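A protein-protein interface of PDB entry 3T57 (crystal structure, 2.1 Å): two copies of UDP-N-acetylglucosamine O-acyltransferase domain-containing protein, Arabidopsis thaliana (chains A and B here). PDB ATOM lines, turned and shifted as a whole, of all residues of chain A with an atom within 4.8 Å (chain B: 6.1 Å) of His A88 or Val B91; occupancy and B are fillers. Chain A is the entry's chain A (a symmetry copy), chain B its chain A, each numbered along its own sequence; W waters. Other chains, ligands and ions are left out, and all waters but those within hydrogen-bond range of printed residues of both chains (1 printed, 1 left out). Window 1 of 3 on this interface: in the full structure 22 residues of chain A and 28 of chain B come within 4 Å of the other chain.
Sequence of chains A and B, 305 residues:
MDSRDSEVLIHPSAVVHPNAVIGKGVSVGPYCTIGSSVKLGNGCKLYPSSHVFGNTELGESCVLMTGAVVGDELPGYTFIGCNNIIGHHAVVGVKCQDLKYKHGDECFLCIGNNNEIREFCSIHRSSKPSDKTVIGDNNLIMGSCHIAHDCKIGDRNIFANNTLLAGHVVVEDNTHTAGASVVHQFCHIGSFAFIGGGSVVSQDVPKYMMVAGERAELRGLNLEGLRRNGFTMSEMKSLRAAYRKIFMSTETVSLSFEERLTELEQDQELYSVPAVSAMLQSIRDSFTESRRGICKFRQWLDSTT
Water W1 bridges O of Gly B71 and NE2 of His A88.
A ring nitrogen (NE2) of His B124 sits close to the side-chain carboxylate of Glu A119 (3.0 Å). The backbone carbonyl oxygen of Gly B67 is in hydrogen-bond range of a ring nitrogen (NE2) of His A89, 2.8 Å away.
Among the printed residues, merely in contact across the chains: Phe A120 with His B89, Thr A66 with Phe B53, Phe A120 with Phe B120, His A89 with His B89, His A88 with Val B94, His A88 with Val B91, Glu A119 with Ser B122, Phe A120 with Cys B121, Phe A120 with Val B91, Thr A66 with Val B69, His A88 with Val B69 and His A89 with Val B91.
Printed residues of chain A that touch a printed residue of chain B: Thr A66, His A88, His A89, Glu A119 and Phe A120. Hydrophobic or aromatic side chains of chain A that line the printed part of chain B: His A88, His A89 and Phe A120. Among the printed residues, 14 pairs touch across the chains. Among the printed residues, no Asp or Glu carboxylate lies within 4 Å of a Lys or Arg side-chain nitrogen of the other chain.
His A88 touches just these residues of chain B: Val B69 (3.8 Å), Val B91 (3.6 Å) and Val B94 (3.5 Å). Val B91 touches just these residues of chain A: His A88 (3.6 Å), His A89 (3.8 Å) and Phe A120 (3.8 Å). Of the printed residues of chain A, His B89 touches His A89 (3.3 Å) and Phe A120 (3.1 Å). Of the printed residues of chain B, Glu A119 touches Ser B122 (3.7 Å) and His B124 (2.8 Å). Of the printed residues of chain B, Thr A66 touches Phe B53 (3.3 Å) and Val B69 (3.8 Å). Ala B90 touches none of the printed residues of chain A. The nearest residue of chain B that does not touch His A88 is Gly B71 (5.2 Å). The nearest printed residue of chain A that does not touch Val B91 is Glu A119 (4.8 Å). The nearest printed residue of chain A that does not touch His B89 is His A88 (6.3 Å).
His A89 touches its own counterpart, His B89. Phe A120 touches His B89, but with the chains exchanged His A89 does not touch Phe B120 (6.3 Å). Phe A120 touches its own counterpart, Phe B120.
N of Ile B123 lies within hydrogen-bond range of O of Val B91 (3.0 Å). N of Phe B53 lies within hydrogen-bond range of O of Val B70. The backbone carbonyl oxygen of Val B69 is in hydrogen-bond range of the backbone NH of Val B92, 2.9 Å away. N of His A89 is in hydrogen-bond range of O of Thr A66, 3.0 Å away. The backbone NH (N) of Val B69 lies within hydrogen-bond range of the backbone carbonyl oxygen (O) of Ala B90 (2.8 Å). The backbone NH of Val B91 sits at hydrogen-bond distance from the backbone carbonyl oxygen of Cys B121 (2.8 Å).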
ATOM      1  N   MET A  65      29.276  11.506 -20.866  1.00  0.00           N
ATOM      2  CA  MET A  65      28.363  10.945 -21.842  1.00  0.00           C
ATOM      3  C   MET A  65      26.918  11.169 -21.397  1.00  0.00           C
ATOM      4  O   MET A  65      26.665  11.528 -20.248  1.00  0.00           O
ATOM      5  CB  MET A  65      28.617   9.441 -22.027  1.00  0.00           C
ATOM      6  CG  MET A  65      30.026   9.079 -22.528  1.00  0.00           C
ATOM      7  SD  MET A  65      30.579  10.108 -23.904  1.00  0.00           S
ATOM      8  CE  MET A  65      29.537   9.543 -25.250  1.00  0.00           C
ATOM      9  N   THR A  66      25.974  10.936 -22.312  1.00  0.00           N
ATOM     10  CA  THR A  66      24.551  11.127 -22.021  1.00  0.00           C
ATOM     11  C   THR A  66      24.112  10.359 -20.785  1.00  0.00           C
ATOM     12  O   THR A  66      24.441   9.176 -20.607  1.00  0.00           O
ATOM     13  CB  THR A  66      23.684  10.762 -23.240  1.00  0.00           C
ATOM     14  OG1 THR A  66      23.965  11.705 -24.282  1.00  0.00           O
ATOM     15  CG2 THR A  66      22.190  10.805 -22.912  1.00  0.00           C
ATOM     16  N   ALA A  68      25.028  10.807 -17.760  1.00  0.00           N
ATOM     17  CA  ALA A  68      26.019  10.793 -16.673  1.00  0.00           C
ATOM     18  C   ALA A  68      25.622  11.808 -15.616  1.00  0.00           C
ATOM     19  O   ALA A  68      25.158  12.905 -15.944  1.00  0.00           O
ATOM     20  CB  ALA A  68      27.452  11.077 -17.194  1.00  0.00           C
ATOM     21  N   ILE A  86      33.460   9.869 -18.280  1.00  0.00           N
ATOM     22  CA  ILE A  86      32.371   9.321 -17.474  1.00  0.00           C
ATOM     23  C   ILE A  86      31.295   8.810 -18.430  1.00  0.00           C
ATOM     24  O   ILE A  86      30.690   9.594 -19.162  1.00  0.00           O
ATOM     25  CB  ILE A  86      31.781  10.399 -16.505  1.00  0.00           C
ATOM     26  CG1 ILE A  86      32.894  11.155 -15.755  1.00  0.00           C
ATOM     27  CG2 ILE A  86      30.760   9.796 -15.542  1.00  0.00           C
ATOM     28  CD1 ILE A  86      33.589  10.405 -14.651  1.00  0.00           C
ATOM     29  N   GLY A  87      31.096   7.492 -18.439  1.00  0.00           N
ATOM     30  CA  GLY A  87      30.201   6.823 -19.377  1.00  0.00           C
ATOM     31  C   GLY A  87      28.717   7.097 -19.208  1.00  0.00           C
ATOM     32  O   GLY A  87      28.285   7.746 -18.244  1.00  0.00           O
ATOM     33  N   HIS A  88      27.943   6.590 -20.162  1.00  0.00           N
ATOM     34  CA  HIS A  88      26.498   6.798 -20.220  1.00  0.00           C
ATOM     35  C   HIS A  88      25.817   6.336 -18.945  1.00  0.00           C
ATOM     36  O   HIS A  88      25.991   5.183 -18.527  1.00  0.00           O
ATOM     37  CB  HIS A  88      25.902   5.999 -21.383  1.00  0.00           C
ATOM     38  CG  HIS A  88      26.450   6.367 -22.725  1.00  0.00           C
ATOM     39  ND1 HIS A  88      27.633   5.851 -23.214  1.00  0.00           N
ATOM     40  CD2 HIS A  88      25.966   7.180 -23.692  1.00  0.00           C
ATOM     41  CE1 HIS A  88      27.861   6.343 -24.421  1.00  0.00           C
ATOM     42  NE2 HIS A  88      26.862   7.148 -24.737  1.00  0.00           N
ATOM     43  N   HIS A  89      25.032   7.226 -18.345  1.00  0.00           N
ATOM     44  CA  HIS A  89      24.275   6.930 -17.127  1.00  0.00           C
ATOM     45  C   HIS A  89      25.109   6.568 -15.904  1.00  0.00           C
ATOM     46  O   HIS A  89      24.548   6.108 -14.920  1.00  0.00           O
ATOM     47  CB  HIS A  89      23.205   5.843 -17.371  1.00  0.00           C
ATOM     48  CG  HIS A  89      22.276   6.155 -18.506  1.00  0.00           C
ATOM     49  ND1 HIS A  89      21.491   7.288 -18.535  1.00  0.00           N
ATOM     50  CD2 HIS A  89      22.016   5.490 -19.655  1.00  0.00           C
ATOM     51  CE1 HIS A  89      20.777   7.301 -19.646  1.00  0.00           C
ATOM     52  NE2 HIS A  89      21.080   6.224 -20.344  1.00  0.00           N
ATOM     53  N   ALA A  90      26.426   6.776 -15.950  1.00  0.00           N
ATOM     54  CA  ALA A  90      27.272   6.547 -14.769  1.00  0.00           C
ATOM     55  C   ALA A  90      26.903   7.550 -13.681  1.00  0.00           C
ATOM     56  O   ALA A  90      26.517   8.698 -13.976  1.00  0.00           O
ATOM     57  CB  ALA A  90      28.766   6.650 -15.119  1.00  0.00           C
ATOM     58  N   GLU A 119      29.716   2.852 -18.662  1.00  0.00           N
ATOM     59  CA  GLU A 119      28.285   3.028 -18.439  1.00  0.00           C
ATOM     60  C   GLU A 119      27.791   2.348 -17.166  1.00  0.00           C
ATOM     61  O   GLU A 119      28.242   1.249 -16.830  1.00  0.00           O
ATOM     62  CB  GLU A 119      27.466   2.543 -19.656  1.00  0.00           C
ATOM     63  CG  GLU A 119      27.769   1.135 -20.149  1.00  0.00           C
ATOM     64  CD  GLU A 119      29.032   1.036 -21.023  1.00  0.00           C
ATOM     65  OE1 GLU A 119      29.695   2.059 -21.309  1.00  0.00           O
ATOM     66  OE2 GLU A 119      29.375  -0.092 -21.409  1.00  0.00           O
ATOM     67  N   PHE A 120      26.842   2.993 -16.489  1.00  0.00           N
ATOM     68  CA  PHE A 120      26.155   2.406 -15.325  1.00  0.00           C
ATOM     69  C   PHE A 120      27.051   2.130 -14.104  1.00  0.00           C
ATOM     70  O   PHE A 120      26.643   1.409 -13.197  1.00  0.00           O
ATOM     71  CB  PHE A 120      25.433   1.101 -15.684  1.00  0.00           C
ATOM     72  CG  PHE A 120      24.661   1.153 -16.976  1.00  0.00           C
ATOM     73  CD1 PHE A 120      23.557   1.992 -17.115  1.00  0.00           C
ATOM     74  CD2 PHE A 120      25.025   0.327 -18.041  1.00  0.00           C
ATOM     75  CE1 PHE A 120      22.831   2.024 -18.316  1.00  0.00           C
ATOM     76  CE2 PHE A 120      24.318   0.351 -19.242  1.00  0.00           C
ATOM     77  CZ  PHE A 120      23.221   1.197 -19.383  1.00  0.00           C
ATOM     78  N   PHE B  53      22.311   8.739 -31.782  1.00  0.00           N
ATOM     79  CA  PHE B  53      23.531   9.451 -32.206  1.00  0.00           C
ATOM     80  C   PHE B  53      24.192   8.740 -33.391  1.00  0.00           C
ATOM     81  O   PHE B  53      23.914   7.562 -33.668  1.00  0.00           O
ATOM     82  CB  PHE B  53      24.580   9.492 -31.078  1.00  0.00           C
ATOM     83  CG  PHE B  53      24.158  10.255 -29.841  1.00  0.00           C
ATOM     84  CD1 PHE B  53      24.241  11.648 -29.800  1.00  0.00           C
ATOM     85  CD2 PHE B  53      23.704   9.577 -28.708  1.00  0.00           C
ATOM     86  CE1 PHE B  53      23.855  12.359 -28.637  1.00  0.00           C
ATOM     87  CE2 PHE B  53      23.333  10.270 -27.538  1.00  0.00           C
ATOM     88  CZ  PHE B  53      23.396  11.655 -27.507  1.00  0.00           C
ATOM     89  N   GLY B  67      15.443   7.273 -21.629  1.00  0.00           N
ATOM     90  CA  GLY B  67      16.847   7.166 -21.269  1.00  0.00           C
ATOM     91  C   GLY B  67      17.656   6.334 -22.247  1.00  0.00           C
ATOM     92  O   GLY B  67      18.889   6.315 -22.162  1.00  0.00           O
ATOM     93  N   ALA B  68      16.984   5.631 -23.163  1.00  0.00           N
ATOM     94  CA  ALA B  68      17.685   4.757 -24.116  1.00  0.00           C
ATOM     95  C   ALA B  68      18.607   5.595 -24.985  1.00  0.00           C
ATOM     96  O   ALA B  68      18.246   6.703 -25.393  1.00  0.00           O
ATOM     97  CB  ALA B  68      16.695   3.946 -24.993  1.00  0.00           C
ATOM     98  N   VAL B  69      19.808   5.076 -25.219  1.00  0.00           N
ATOM     99  CA  VAL B  69      20.807   5.719 -26.068  1.00  0.00           C
ATOM    100  C   VAL B  69      21.226   4.708 -27.137  1.00  0.00           C
ATOM    101  O   VAL B  69      21.695   3.606 -26.827  1.00  0.00           O
ATOM    102  CB  VAL B  69      22.040   6.212 -25.267  1.00  0.00           C
ATOM    103  CG1 VAL B  69      23.109   6.796 -26.214  1.00  0.00           C
ATOM    104  CG2 VAL B  69      21.634   7.278 -24.215  1.00  0.00           C
ATOM    105  N   VAL B  70      21.027   5.071 -28.394  1.00  0.00           N
ATOM    106  CA  VAL B  70      21.398   4.210 -29.496  1.00  0.00           C
ATOM    107  C   VAL B  70      22.386   4.957 -30.380  1.00  0.00           C
ATOM    108  O   VAL B  70      22.140   6.100 -30.778  1.00  0.00           O
ATOM    109  CB  VAL B  70      20.177   3.755 -30.315  1.00  0.00           C
ATOM    110  CG1 VAL B  70      20.611   2.822 -31.448  1.00  0.00           C
ATOM    111  CG2 VAL B  70      19.128   3.054 -29.413  1.00  0.00           C
ATOM    112  N   GLY B  71      23.518   4.312 -30.650  1.00  0.00           N
ATOM    113  CA  GLY B  71      24.540   4.873 -31.513  1.00  0.00           C
ATOM    114  C   GLY B  71      25.491   5.751 -30.720  1.00  0.00           C
ATOM    115  O   GLY B  71      25.213   6.126 -29.566  1.00  0.00           O
ATOM    116  N   ASP B  72      26.632   6.043 -31.345  1.00  0.00           N
ATOM    117  CA  ASP B  72      27.540   7.089 -30.892  1.00  0.00           C
ATOM    118  C   ASP B  72      28.310   7.662 -32.089  1.00  0.00           C
ATOM    119  O   ASP B  72      28.302   7.082 -33.190  1.00  0.00           O
ATOM    120  CB  ASP B  72      28.453   6.628 -29.726  1.00  0.00           C
ATOM    121  CG  ASP B  72      29.680   5.853 -30.171  1.00  0.00           C
ATOM    122  OD1 ASP B  72      29.856   5.579 -31.384  1.00  0.00           O
ATOM    123  OD2 ASP B  72      30.482   5.496 -29.273  1.00  0.00           O
ATOM    124  N   ILE B  86      14.009  -1.171 -27.303  1.00  0.00           N
ATOM    125  CA  ILE B  86      15.205  -0.824 -26.537  1.00  0.00           C
ATOM    126  C   ILE B  86      14.748  -0.250 -25.197  1.00  0.00           C
ATOM    127  O   ILE B  86      14.113   0.805 -25.156  1.00  0.00           O
ATOM    128  CB  ILE B  86      16.094   0.210 -27.306  1.00  0.00           C
ATOM    129  CG1 ILE B  86      16.301  -0.206 -28.775  1.00  0.00           C
ATOM    130  CG2 ILE B  86      17.424   0.450 -26.594  1.00  0.00           C
ATOM    131  CD1 ILE B  86      17.247  -1.349 -29.022  1.00  0.00           C
ATOM    132  N   GLY B  87      15.046  -0.972 -24.117  1.00  0.00           N
ATOM    133  CA  GLY B  87      14.579  -0.639 -22.776  1.00  0.00           C
ATOM    134  C   GLY B  87      15.154   0.621 -22.153  1.00  0.00           C
ATOM    135  O   GLY B  87      16.068   1.254 -22.701  1.00  0.00           O
ATOM    136  N   HIS B  89      17.097   3.331 -20.359  1.00  0.00           N
ATOM    137  CA  HIS B  89      18.525   3.549 -20.115  1.00  0.00           C
ATOM    138  C   HIS B  89      19.466   2.545 -20.769  1.00  0.00           C
ATOM    139  O   HIS B  89      20.645   2.537 -20.442  1.00  0.00           O
ATOM    140  CB  HIS B  89      18.836   3.652 -18.605  1.00  0.00           C
ATOM    141  CG  HIS B  89      18.016   4.684 -17.890  1.00  0.00           C
ATOM    142  ND1 HIS B  89      18.028   6.017 -18.239  1.00  0.00           N
ATOM    143  CD2 HIS B  89      17.151   4.575 -16.855  1.00  0.00           C
ATOM    144  CE1 HIS B  89      17.217   6.688 -17.441  1.00  0.00           C
ATOM    145  NE2 HIS B  89      16.670   5.836 -16.596  1.00  0.00           N
ATOM    146  N   ALA B  90      18.969   1.712 -21.686  1.00  0.00           N
ATOM    147  CA  ALA B  90      19.843   0.792 -22.429  1.00  0.00           C
ATOM    148  C   ALA B  90      20.788   1.598 -23.315  1.00  0.00           C
ATOM    149  O   ALA B  90      20.423   2.678 -23.819  1.00  0.00           O
ATOM    150  CB  ALA B  90      19.026  -0.203 -23.269  1.00  0.00           C
ATOM    151  N   VAL B  91      22.004   1.092 -23.491  1.00  0.00           N
ATOM    152  CA  VAL B  91      23.029   1.795 -24.256  1.00  0.00           C
ATOM    153  C   VAL B  91      23.501   0.837 -25.353  1.00  0.00           C
ATOM    154  O   VAL B  91      24.092  -0.207 -25.076  1.00  0.00           O
ATOM    155  CB  VAL B  91      24.180   2.283 -23.318  1.00  0.00           C
ATOM    156  CG1 VAL B  91      25.381   2.766 -24.100  1.00  0.00           C
ATOM    157  CG2 VAL B  91      23.674   3.419 -22.422  1.00  0.00           C
ATOM    158  N   VAL B  92      23.172   1.168 -26.595  1.00  0.00           N
ATOM    159  CA  VAL B  92      23.267   0.203 -27.691  1.00  0.00           C
ATOM    160  C   VAL B  92      24.038   0.824 -28.840  1.00  0.00           C
ATOM    161  O   VAL B  92      23.592   1.805 -29.423  1.00  0.00           O
ATOM    162  CB  VAL B  92      21.861  -0.212 -28.173  1.00  0.00           C
ATOM    163  CG1 VAL B  92      21.929  -1.164 -29.398  1.00  0.00           C
ATOM    164  CG2 VAL B  92      21.096  -0.884 -27.051  1.00  0.00           C
ATOM    165  N   GLY B  93      25.196   0.255 -29.153  1.00  0.00           N
ATOM    166  CA  GLY B  93      26.028   0.727 -30.272  1.00  0.00           C
ATOM    167  C   GLY B  93      27.062   1.760 -29.866  1.00  0.00           C
ATOM    168  O   GLY B  93      27.324   2.698 -30.619  1.00  0.00           O
ATOM    169  N   VAL B  94      27.655   1.585 -28.686  1.00  0.00           N
ATOM    170  CA  VAL B  94      28.705   2.486 -28.198  1.00  0.00           C
ATOM    171  C   VAL B  94      30.095   1.845 -28.265  1.00  0.00           C
ATOM    172  O   VAL B  94      30.218   0.631 -28.425  1.00  0.00           O
ATOM    173  CB  VAL B  94      28.433   2.953 -26.729  1.00  0.00           C
ATOM    174  CG1 VAL B  94      27.139   3.731 -26.663  1.00  0.00           C
ATOM    175  CG2 VAL B  94      28.405   1.768 -25.777  1.00  0.00           C
ATOM    176  N   PHE B 120      19.034  -1.031 -18.995  1.00  0.00           N
ATOM    177  CA  PHE B 120      20.442  -1.052 -18.562  1.00  0.00           C
ATOM    178  C   PHE B 120      21.345  -2.044 -19.316  1.00  0.00           C
ATOM    179  O   PHE B 120      22.452  -2.328 -18.862  1.00  0.00           O
ATOM    180  CB  PHE B 120      20.576  -1.336 -17.062  1.00  0.00           C
ATOM    181  CG  PHE B 120      19.607  -0.575 -16.196  1.00  0.00           C
ATOM    182  CD1 PHE B 120      19.673   0.814 -16.103  1.00  0.00           C
ATOM    183  CD2 PHE B 120      18.654  -1.261 -15.442  1.00  0.00           C
ATOM    184  CE1 PHE B 120      18.778   1.518 -15.281  1.00  0.00           C
ATOM    185  CE2 PHE B 120      17.755  -0.578 -14.626  1.00  0.00           C
ATOM    186  CZ  PHE B 120      17.814   0.811 -14.542  1.00  0.00           C
ATOM    187  N   CYS B 121      20.896  -2.566 -20.453  1.00  0.00           N
ATOM    188  CA  CYS B 121      21.798  -3.371 -21.271  1.00  0.00           C
ATOM    189  C   CYS B 121      22.863  -2.494 -21.927  1.00  0.00           C
ATOM    190  O   CYS B 121      22.656  -1.293 -22.169  1.00  0.00           O
ATOM    191  CB  CYS B 121      21.033  -4.147 -22.345  1.00  0.00           C
ATOM    192  SG  CYS B 121      20.095  -5.523 -21.701  1.00  0.00           S
ATOM    193  N   SER B 122      24.015  -3.087 -22.194  1.00  0.00           N
ATOM    194  CA  SER B 122      25.050  -2.388 -22.934  1.00  0.00           C
ATOM    195  C   SER B 122      25.547  -3.318 -24.027  1.00  0.00           C
ATOM    196  O   SER B 122      25.974  -4.454 -23.765  1.00  0.00           O
ATOM    197  CB  SER B 122      26.197  -1.926 -22.032  1.00  0.00           C
ATOM    198  OG  SER B 122      26.753  -3.025 -21.346  1.00  0.00           O
ATOM    199  N   ILE B 123      25.428  -2.833 -25.255  1.00  0.00           N
ATOM    200  CA  ILE B 123      25.800  -3.581 -26.434  1.00  0.00           C
ATOM    201  C   ILE B 123      26.826  -2.741 -27.149  1.00  0.00           C
ATOM    202  O   ILE B 123      26.556  -1.575 -27.504  1.00  0.00           O
ATOM    203  CB  ILE B 123      24.580  -3.866 -27.332  1.00  0.00           C
ATOM    204  CG1 ILE B 123      23.514  -4.623 -26.518  1.00  0.00           C
ATOM    205  CG2 ILE B 123      25.009  -4.676 -28.592  1.00  0.00           C
ATOM    206  CD1 ILE B 123      22.239  -4.944 -27.266  1.00  0.00           C
ATOM    207  N   HIS B 124      28.014  -3.314 -27.318  1.00  0.00           N
ATOM    208  CA  HIS B 124      29.167  -2.555 -27.817  1.00  0.00           C
ATOM    209  C   HIS B 124      29.457  -2.823 -29.276  1.00  0.00           C
ATOM    210  O   HIS B 124      29.253  -3.927 -29.769  1.00  0.00           O
ATOM    211  CB  HIS B 124      30.433  -2.845 -26.988  1.00  0.00           C
ATOM    212  CG  HIS B 124      30.309  -2.456 -25.547  1.00  0.00           C
ATOM    213  ND1 HIS B 124      30.633  -1.202 -25.084  1.00  0.00           N
ATOM    214  CD2 HIS B 124      29.872  -3.150 -24.469  1.00  0.00           C
ATOM    215  CE1 HIS B 124      30.416  -1.139 -23.782  1.00  0.00           C
ATOM    216  NE2 HIS B 124      29.952  -2.307 -23.384  1.00  0.00           N
HETATM  217  O   HOH W   1      26.443   7.659 -27.513  1.00  0.00           O
